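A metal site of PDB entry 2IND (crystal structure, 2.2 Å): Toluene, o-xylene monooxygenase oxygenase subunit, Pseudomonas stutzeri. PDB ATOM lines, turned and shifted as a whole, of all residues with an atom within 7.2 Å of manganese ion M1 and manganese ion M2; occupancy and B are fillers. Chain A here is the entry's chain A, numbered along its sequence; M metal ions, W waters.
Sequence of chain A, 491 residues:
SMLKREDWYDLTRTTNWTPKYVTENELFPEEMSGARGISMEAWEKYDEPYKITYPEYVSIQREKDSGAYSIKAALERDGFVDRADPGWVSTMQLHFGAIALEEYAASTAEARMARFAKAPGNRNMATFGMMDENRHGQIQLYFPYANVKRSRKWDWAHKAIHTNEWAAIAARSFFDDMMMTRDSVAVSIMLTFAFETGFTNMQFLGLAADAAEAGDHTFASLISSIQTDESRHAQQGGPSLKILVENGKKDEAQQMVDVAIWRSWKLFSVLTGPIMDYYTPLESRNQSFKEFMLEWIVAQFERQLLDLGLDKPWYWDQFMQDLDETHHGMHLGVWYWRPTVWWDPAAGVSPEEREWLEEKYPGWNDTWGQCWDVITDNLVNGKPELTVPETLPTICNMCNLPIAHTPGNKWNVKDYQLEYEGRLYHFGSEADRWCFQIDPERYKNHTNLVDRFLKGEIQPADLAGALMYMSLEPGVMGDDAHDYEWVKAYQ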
ATOM      1  N   GLU A 102      11.069 -19.400  35.607  1.00  0.00           N
ATOM      2  CA  GLU A 102      11.939 -19.015  34.491  1.00  0.00           C
ATOM      3  C   GLU A 102      11.303 -19.621  33.229  1.00  0.00           C
ATOM      4  O   GLU A 102      11.377 -19.055  32.151  1.00  0.00           O
ATOM      5  CB  GLU A 102      13.374 -19.513  34.730  1.00  0.00           C
ATOM      6  CG  GLU A 102      14.078 -18.814  35.910  1.00  0.00           C
ATOM      7  CD  GLU A 102      14.358 -17.329  35.658  1.00  0.00           C
ATOM      8  OE1 GLU A 102      13.665 -16.705  34.842  1.00  0.00           O
ATOM      9  OE2 GLU A 102      15.272 -16.773  36.301  1.00  0.00           O
ATOM     10  N   GLU A 103      10.637 -20.764  33.381  1.00  0.00           N
ATOM     11  CA  GLU A 103       9.937 -21.370  32.244  1.00  0.00           C
ATOM     12  C   GLU A 103       8.881 -20.367  31.773  1.00  0.00           C
ATOM     13  O   GLU A 103       8.744 -20.083  30.569  1.00  0.00           O
ATOM     14  CB  GLU A 103       9.250 -22.673  32.655  1.00  0.00           C
ATOM     15  CG  GLU A 103      10.181 -23.866  32.878  1.00  0.00           C
ATOM     16  CD  GLU A 103      10.583 -24.552  31.571  1.00  0.00           C
ATOM     17  OE1 GLU A 103      11.028 -25.710  31.620  1.00  0.00           O
ATOM     18  OE2 GLU A 103      10.463 -23.905  30.510  1.00  0.00           O
ATOM     19  N   TYR A 104       8.119 -19.831  32.729  1.00  0.00           N
ATOM     20  CA  TYR A 104       7.060 -18.876  32.425  1.00  0.00           C
ATOM     21  C   TYR A 104       7.617 -17.599  31.809  1.00  0.00           C
ATOM     22  O   TYR A 104       7.035 -17.011  30.910  1.00  0.00           O
ATOM     23  CB  TYR A 104       6.260 -18.526  33.686  1.00  0.00           C
ATOM     24  CG  TYR A 104       5.100 -17.589  33.406  1.00  0.00           C
ATOM     25  CD1 TYR A 104       3.960 -18.027  32.741  1.00  0.00           C
ATOM     26  CD2 TYR A 104       5.160 -16.254  33.778  1.00  0.00           C
ATOM     27  CE1 TYR A 104       2.901 -17.161  32.444  1.00  0.00           C
ATOM     28  CE2 TYR A 104       4.114 -15.367  33.495  1.00  0.00           C
ATOM     29  CZ  TYR A 104       2.989 -15.827  32.818  1.00  0.00           C
ATOM     30  OH  TYR A 104       1.972 -14.941  32.523  1.00  0.00           O
ATOM     31  N   ALA A 106      10.180 -17.414  30.022  1.00  0.00           N
ATOM     32  CA  ALA A 106      10.603 -17.744  28.652  1.00  0.00           C
ATOM     33  C   ALA A 106       9.493 -17.488  27.634  1.00  0.00           C
ATOM     34  O   ALA A 106       9.788 -17.283  26.441  1.00  0.00           O
ATOM     35  CB  ALA A 106      11.058 -19.203  28.583  1.00  0.00           C
ATOM     36  N   GLU A 110       9.879 -15.596  24.208  1.00  0.00           N
ATOM     37  CA  GLU A 110       9.363 -16.071  22.936  1.00  0.00           C
ATOM     38  C   GLU A 110       8.507 -14.992  22.294  1.00  0.00           C
ATOM     39  O   GLU A 110       8.591 -14.738  21.084  1.00  0.00           O
ATOM     40  CB  GLU A 110       8.546 -17.352  23.139  1.00  0.00           C
ATOM     41  CG  GLU A 110       9.369 -18.613  23.396  1.00  0.00           C
ATOM     42  CD  GLU A 110      10.050 -19.193  22.141  1.00  0.00           C
ATOM     43  OE1 GLU A 110       9.661 -18.834  21.008  1.00  0.00           O
ATOM     44  OE2 GLU A 110      10.976 -20.030  22.299  1.00  0.00           O
ATOM     45  N   GLY A 129       6.192 -21.415  20.490  1.00  0.00           N
ATOM     46  CA  GLY A 129       7.142 -21.585  21.576  1.00  0.00           C
ATOM     47  C   GLY A 129       6.638 -20.855  22.809  1.00  0.00           C
ATOM     48  O   GLY A 129       6.828 -21.293  23.964  1.00  0.00           O
ATOM     49  N   ASP A 132       4.365 -23.012  24.396  1.00  0.00           N
ATOM     50  CA  ASP A 132       5.043 -24.131  25.052  1.00  0.00           C
ATOM     51  C   ASP A 132       5.524 -23.765  26.459  1.00  0.00           C
ATOM     52  O   ASP A 132       5.339 -24.522  27.411  1.00  0.00           O
ATOM     53  CB  ASP A 132       6.291 -24.612  24.263  1.00  0.00           C
ATOM     54  CG  ASP A 132       5.943 -25.262  22.923  1.00  0.00           C
ATOM     55  OD1 ASP A 132       4.844 -25.839  22.783  1.00  0.00           O
ATOM     56  OD2 ASP A 132       6.810 -25.222  22.026  1.00  0.00           O
ATOM     57  N   GLU A 133       6.166 -22.610  26.582  1.00  0.00           N
ATOM     58  CA  GLU A 133       6.689 -22.184  27.865  1.00  0.00           C
ATOM     59  C   GLU A 133       5.553 -21.819  28.820  1.00  0.00           C
ATOM     60  O   GLU A 133       5.722 -21.851  30.041  1.00  0.00           O
ATOM     61  CB  GLU A 133       7.619 -20.982  27.675  1.00  0.00           C
ATOM     62  CG  GLU A 133       8.651 -21.131  26.541  1.00  0.00           C
ATOM     63  CD  GLU A 133       9.788 -22.086  26.842  1.00  0.00           C
ATOM     64  OE1 GLU A 133      10.899 -21.822  26.340  1.00  0.00           O
ATOM     65  OE2 GLU A 133       9.605 -23.102  27.559  1.00  0.00           O
ATOM     66  N   ASN A 134       4.400 -21.465  28.275  1.00  0.00           N
ATOM     67  CA  ASN A 134       3.250 -21.141  29.111  1.00  0.00           C
ATOM     68  C   ASN A 134       2.882 -22.484  29.765  1.00  0.00           C
ATOM     69  O   ASN A 134       2.634 -22.558  30.972  1.00  0.00           O
ATOM     70  CB  ASN A 134       2.099 -20.581  28.251  1.00  0.00           C
ATOM     71  CG  ASN A 134       0.818 -20.371  29.039  1.00  0.00           C
ATOM     72  OD1 ASN A 134      -0.036 -21.261  29.109  1.00  0.00           O
ATOM     73  ND2 ASN A 134       0.674 -19.199  29.646  1.00  0.00           N
ATOM     74  N   ARG A 135       2.895 -23.542  28.956  1.00  0.00           N
ATOM     75  CA  ARG A 135       2.593 -24.888  29.444  1.00  0.00           C
ATOM     76  C   ARG A 135       3.612 -25.322  30.492  1.00  0.00           C
ATOM     77  O   ARG A 135       3.261 -25.818  31.570  1.00  0.00           O
ATOM     78  CB  ARG A 135       2.627 -25.904  28.291  1.00  0.00           C
ATOM     79  CG  ARG A 135       2.342 -27.343  28.745  1.00  0.00           C
ATOM     80  CD  ARG A 135       2.772 -28.377  27.724  1.00  0.00           C
ATOM     81  NE  ARG A 135       2.368 -29.719  28.141  1.00  0.00           N
ATOM     82  CZ  ARG A 135       3.058 -30.841  27.889  1.00  0.00           C
ATOM     83  NH1 ARG A 135       4.209 -30.791  27.222  1.00  0.00           N
ATOM     84  NH2 ARG A 135       2.602 -32.001  28.324  1.00  0.00           N
ATOM     85  N   HIS A 136       4.883 -25.144  30.163  1.00  0.00           N
ATOM     86  CA  HIS A 136       5.975 -25.531  31.048  1.00  0.00           C
ATOM     87  C   HIS A 136       5.925 -24.801  32.386  1.00  0.00           C
ATOM     88  O   HIS A 136       6.144 -25.388  33.434  1.00  0.00           O
ATOM     89  CB  HIS A 136       7.311 -25.294  30.334  1.00  0.00           C
ATOM     90  CG  HIS A 136       7.449 -26.087  29.070  1.00  0.00           C
ATOM     91  ND1 HIS A 136       8.559 -26.038  28.265  1.00  0.00           N
ATOM     92  CD2 HIS A 136       6.584 -26.960  28.477  1.00  0.00           C
ATOM     93  CE1 HIS A 136       8.386 -26.845  27.225  1.00  0.00           C
ATOM     94  NE2 HIS A 136       7.201 -27.411  27.335  1.00  0.00           N
ATOM     95  N   GLY A 137       5.626 -23.510  32.357  1.00  0.00           N
ATOM     96  CA  GLY A 137       5.540 -22.788  33.608  1.00  0.00           C
ATOM     97  C   GLY A 137       4.369 -23.308  34.426  1.00  0.00           C
ATOM     98  O   GLY A 137       4.505 -23.552  35.626  1.00  0.00           O
ATOM     99  N   GLN A 140       4.682 -27.142  35.634  1.00  0.00           N
ATOM    100  CA  GLN A 140       5.707 -27.318  36.654  1.00  0.00           C
ATOM    101  C   GLN A 140       5.384 -26.563  37.939  1.00  0.00           C
ATOM    102  O   GLN A 140       6.244 -26.379  38.821  1.00  0.00           O
ATOM    103  CB  GLN A 140       7.083 -26.967  36.097  1.00  0.00           C
ATOM    104  CG  GLN A 140       7.358 -27.865  34.907  1.00  0.00           C
ATOM    105  CD  GLN A 140       8.794 -27.856  34.459  1.00  0.00           C
ATOM    106  OE1 GLN A 140       9.601 -28.658  34.934  1.00  0.00           O
ATOM    107  NE2 GLN A 140       9.132 -26.945  33.546  1.00  0.00           N
ATOM    108  N   LEU A 191      19.303 -18.091  23.522  1.00  0.00           N
ATOM    109  CA  LEU A 191      18.376 -18.969  24.233  1.00  0.00           C
ATOM    110  C   LEU A 191      18.050 -20.298  23.560  1.00  0.00           C
ATOM    111  O   LEU A 191      18.374 -21.358  24.098  1.00  0.00           O
ATOM    112  CB  LEU A 191      17.064 -18.228  24.522  1.00  0.00           C
ATOM    113  CG  LEU A 191      15.923 -19.076  25.112  1.00  0.00           C
ATOM    114  CD1 LEU A 191      16.321 -19.617  26.479  1.00  0.00           C
ATOM    115  CD2 LEU A 191      14.650 -18.230  25.209  1.00  0.00           C
ATOM    116  N   THR A 192      17.418 -20.274  22.391  1.00  0.00           N
ATOM    117  CA  THR A 192      17.042 -21.513  21.729  1.00  0.00           C
ATOM    118  C   THR A 192      18.198 -22.343  21.211  1.00  0.00           C
ATOM    119  O   THR A 192      18.187 -23.568  21.323  1.00  0.00           O
ATOM    120  CB  THR A 192      16.018 -21.268  20.568  1.00  0.00           C
ATOM    121  OG1 THR A 192      16.633 -20.497  19.526  1.00  0.00           O
ATOM    122  CG2 THR A 192      14.777 -20.528  21.088  1.00  0.00           C
ATOM    123  N   PHE A 195      21.366 -22.337  24.775  1.00  0.00           N
ATOM    124  CA  PHE A 195      20.874 -22.993  25.992  1.00  0.00           C
ATOM    125  C   PHE A 195      19.966 -24.204  25.815  1.00  0.00           C
ATOM    126  O   PHE A 195      20.200 -25.247  26.432  1.00  0.00           O
ATOM    127  CB  PHE A 195      20.177 -21.961  26.877  1.00  0.00           C
ATOM    128  CG  PHE A 195      19.713 -22.519  28.195  1.00  0.00           C
ATOM    129  CD1 PHE A 195      20.644 -22.910  29.156  1.00  0.00           C
ATOM    130  CD2 PHE A 195      18.358 -22.630  28.485  1.00  0.00           C
ATOM    131  CE1 PHE A 195      20.221 -23.413  30.393  1.00  0.00           C
ATOM    132  CE2 PHE A 195      17.921 -23.123  29.721  1.00  0.00           C
ATOM    133  CZ  PHE A 195      18.852 -23.516  30.668  1.00  0.00           C
ATOM    134  N   GLU A 196      18.938 -24.083  24.991  1.00  0.00           N
ATOM    135  CA  GLU A 196      18.008 -25.194  24.811  1.00  0.00           C
ATOM    136  C   GLU A 196      18.564 -26.316  23.940  1.00  0.00           C
ATOM    137  O   GLU A 196      18.717 -27.454  24.381  1.00  0.00           O
ATOM    138  CB  GLU A 196      16.685 -24.673  24.228  1.00  0.00           C
ATOM    139  CG  GLU A 196      15.971 -23.659  25.142  1.00  0.00           C
ATOM    140  CD  GLU A 196      14.773 -22.984  24.476  1.00  0.00           C
ATOM    141  OE1 GLU A 196      14.876 -22.648  23.282  1.00  0.00           O
ATOM    142  OE2 GLU A 196      13.740 -22.772  25.150  1.00  0.00           O
ATOM    143  N   THR A 200      19.745 -28.008  27.671  1.00  0.00           N
ATOM    144  CA  THR A 200      18.500 -28.572  28.196  1.00  0.00           C
ATOM    145  C   THR A 200      17.805 -29.662  27.390  1.00  0.00           C
ATOM    146  O   THR A 200      17.161 -30.540  27.969  1.00  0.00           O
ATOM    147  CB  THR A 200      17.489 -27.438  28.478  1.00  0.00           C
ATOM    148  OG1 THR A 200      17.124 -26.785  27.260  1.00  0.00           O
ATOM    149  CG2 THR A 200      18.121 -26.429  29.401  1.00  0.00           C
ATOM    150  N   ASN A 201      17.933 -29.618  26.065  1.00  0.00           N
ATOM    151  CA  ASN A 201      17.303 -30.640  25.235  1.00  0.00           C
ATOM    152  C   ASN A 201      17.769 -32.028  25.673  1.00  0.00           C
ATOM    153  O   ASN A 201      16.976 -32.963  25.800  1.00  0.00           O
ATOM    154  CB  ASN A 201      17.643 -30.416  23.759  1.00  0.00           C
ATOM    155  CG  ASN A 201      16.569 -29.617  23.013  1.00  0.00           C
ATOM    156  OD1 ASN A 201      15.742 -28.929  23.611  1.00  0.00           O
ATOM    157  ND2 ASN A 201      16.591 -29.714  21.686  1.00  0.00           N
ATOM    158  N   PHE A 204      17.254 -32.750  29.921  1.00  0.00           N
ATOM    159  CA  PHE A 204      15.915 -33.241  30.229  1.00  0.00           C
ATOM    160  C   PHE A 204      15.743 -34.696  29.860  1.00  0.00           C
ATOM    161  O   PHE A 204      14.954 -35.412  30.474  1.00  0.00           O
ATOM    162  CB  PHE A 204      14.875 -32.390  29.502  1.00  0.00           C
ATOM    163  CG  PHE A 204      14.364 -31.223  30.315  1.00  0.00           C
ATOM    164  CD1 PHE A 204      15.234 -30.456  31.087  1.00  0.00           C
ATOM    165  CD2 PHE A 204      13.016 -30.896  30.308  1.00  0.00           C
ATOM    166  CE1 PHE A 204      14.762 -29.383  31.847  1.00  0.00           C
ATOM    167  CE2 PHE A 204      12.539 -29.824  31.060  1.00  0.00           C
ATOM    168  CZ  PHE A 204      13.408 -29.067  31.833  1.00  0.00           C
ATOM    169  N   ILE A 226       7.601 -32.489  28.421  1.00  0.00           N
ATOM    170  CA  ILE A 226       8.133 -31.148  28.238  1.00  0.00           C
ATOM    171  C   ILE A 226       9.229 -31.170  27.183  1.00  0.00           C
ATOM    172  O   ILE A 226       9.309 -30.306  26.315  1.00  0.00           O
ATOM    173  CB  ILE A 226       8.752 -30.600  29.546  1.00  0.00           C
ATOM    174  CG1 ILE A 226       7.701 -30.543  30.665  1.00  0.00           C
ATOM    175  CG2 ILE A 226       9.350 -29.232  29.315  1.00  0.00           C
ATOM    176  CD1 ILE A 226       6.504 -29.722  30.308  1.00  0.00           C
ATOM    177  N   ASP A 229       8.373 -30.755  23.524  1.00  0.00           N
ATOM    178  CA  ASP A 229       8.012 -29.395  23.102  1.00  0.00           C
ATOM    179  C   ASP A 229       9.290 -28.591  22.822  1.00  0.00           C
ATOM    180  O   ASP A 229       9.356 -27.836  21.856  1.00  0.00           O
ATOM    181  CB  ASP A 229       7.219 -28.638  24.187  1.00  0.00           C
ATOM    182  CG  ASP A 229       5.920 -29.333  24.570  1.00  0.00           C
ATOM    183  OD1 ASP A 229       5.400 -30.142  23.773  1.00  0.00           O
ATOM    184  OD2 ASP A 229       5.406 -29.045  25.675  1.00  0.00           O
ATOM    185  N   GLU A 230      10.266 -28.737  23.709  1.00  0.00           N
ATOM    186  CA  GLU A 230      11.541 -28.039  23.616  1.00  0.00           C
ATOM    187  C   GLU A 230      12.265 -28.421  22.332  1.00  0.00           C
ATOM    188  O   GLU A 230      12.796 -27.574  21.614  1.00  0.00           O
ATOM    189  CB  GLU A 230      12.429 -28.401  24.814  1.00  0.00           C
ATOM    190  CG  GLU A 230      11.970 -27.843  26.155  1.00  0.00           C
ATOM    191  CD  GLU A 230      11.999 -26.325  26.192  1.00  0.00           C
ATOM    192  OE1 GLU A 230      10.920 -25.712  26.376  1.00  0.00           O
ATOM    193  OE2 GLU A 230      13.081 -25.743  26.025  1.00  0.00           O
ATOM    194  N   SER A 231      12.276 -29.716  22.068  1.00  0.00           N
ATOM    195  CA  SER A 231      12.903 -30.271  20.885  1.00  0.00           C
ATOM    196  C   SER A 231      12.348 -29.580  19.645  1.00  0.00           C
ATOM    197  O   SER A 231      12.997 -29.531  18.606  1.00  0.00           O
ATOM    198  CB  SER A 231      12.628 -31.782  20.826  1.00  0.00           C
ATOM    199  OG  SER A 231      13.142 -32.357  19.638  1.00  0.00           O
ATOM    200  N   HIS A 233      10.576 -26.072  19.548  1.00  0.00           N
ATOM    201  CA  HIS A 233      10.883 -24.645  19.438  1.00  0.00           C
ATOM    202  C   HIS A 233      12.351 -24.246  19.600  1.00  0.00           C
ATOM    203  O   HIS A 233      12.721 -23.115  19.311  1.00  0.00           O
ATOM    204  CB  HIS A 233      10.012 -23.798  20.398  1.00  0.00           C
ATOM    205  CG  HIS A 233      10.282 -24.031  21.854  1.00  0.00           C
ATOM    206  ND1 HIS A 233       9.381 -24.669  22.683  1.00  0.00           N
ATOM    207  CD2 HIS A 233      11.331 -23.684  22.635  1.00  0.00           C
ATOM    208  CE1 HIS A 233       9.861 -24.700  23.908  1.00  0.00           C
ATOM    209  NE2 HIS A 233      11.040 -24.104  23.909  1.00  0.00           N
ATOM    210  N   ALA A 234      13.174 -25.180  20.058  1.00  0.00           N
ATOM    211  CA  ALA A 234      14.599 -24.910  20.243  1.00  0.00           C
ATOM    212  C   ALA A 234      15.307 -24.664  18.908  1.00  0.00           C
ATOM    213  O   ALA A 234      16.402 -24.132  18.881  1.00  0.00           O
ATOM    214  CB  ALA A 234      15.260 -26.084  20.959  1.00  0.00           C
HETATM  215 MN    MN M   1      10.359 -24.854  28.455  1.00  0.00          MN
HETATM  216 MN    MN M   2      12.129 -23.758  25.929  1.00  0.00          MN
HETATM  217  O   HOH W   1      12.752 -23.534  28.052  1.00  0.00           O
HETATM  218  O   HOH W   2      11.483 -26.398  29.286  1.00  0.00           O
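OE2 of Glu 196 is bound to manganese ion M2 (2.0 Å). The side-chain carboxylate (OE2) of Glu 230 binds manganese ion M2, 2.2 Å away. Manganese ion M2 is bound by water W1 (2.2 Å). A ring nitrogen (NE2) of His 233 binds manganese ion M2 (2.3 Å). Manganese ion M2 is bound by OE1 of Glu 133 (2.3 Å). The side-chain carboxylate (OE1) of Glu 230 binds manganese ion M2. Manganese ion M2 has six donor atoms within binding distance.
N of Glu 196 sits at hydrogen-bond distance from O of Leu 191, 2.9 Å away. O of Glu 196 sits close to OG1 of Thr 200 (3.4 Å). A ring nitrogen (NE2) of His 136 sits close to the backbone carbonyl oxygen of Asp 132 (3.4 Å). NE2 of Gln 140 sits close to O of His 136 (3.4 Å). A ring nitrogen (NE2) of His 136 sits at hydrogen-bond distance from the side-chain carboxylate (OD2) of Asp 229 (2.9 Å). The side-chain carboxylate (OE1) of Glu 103 is in hydrogen-bond range of the side-chain amide nitrogen (NE2) of Gln 140, at 3.0 Å. OD2 of Asp 132 lies within hydrogen-bond range of ND1 of His 233, at 2.7 Å. ND1 of His 233 is in hydrogen-bond range of O of Asp 229.
Within 4 Å of manganese ion M2: Glu 133, Glu 196, Glu 230 and His 233. The nearest printed residue that does not touch manganese ion M2 is His 136 (4.8 Å).
Of the 26 residues printed, 4 come within 4 Å of manganese ion M1.
Manganese ion M1 is bound by water W2, the side-chain carboxylate (OE2) of Glu 133, a ring nitrogen (ND1) of His 136, the side-chain carboxylate (OE2) of Glu 103 and the side-chain carboxylate (OE1) of Glu 230. Slightly farther from manganese ion M1 lies water W1 (2.8 Å).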
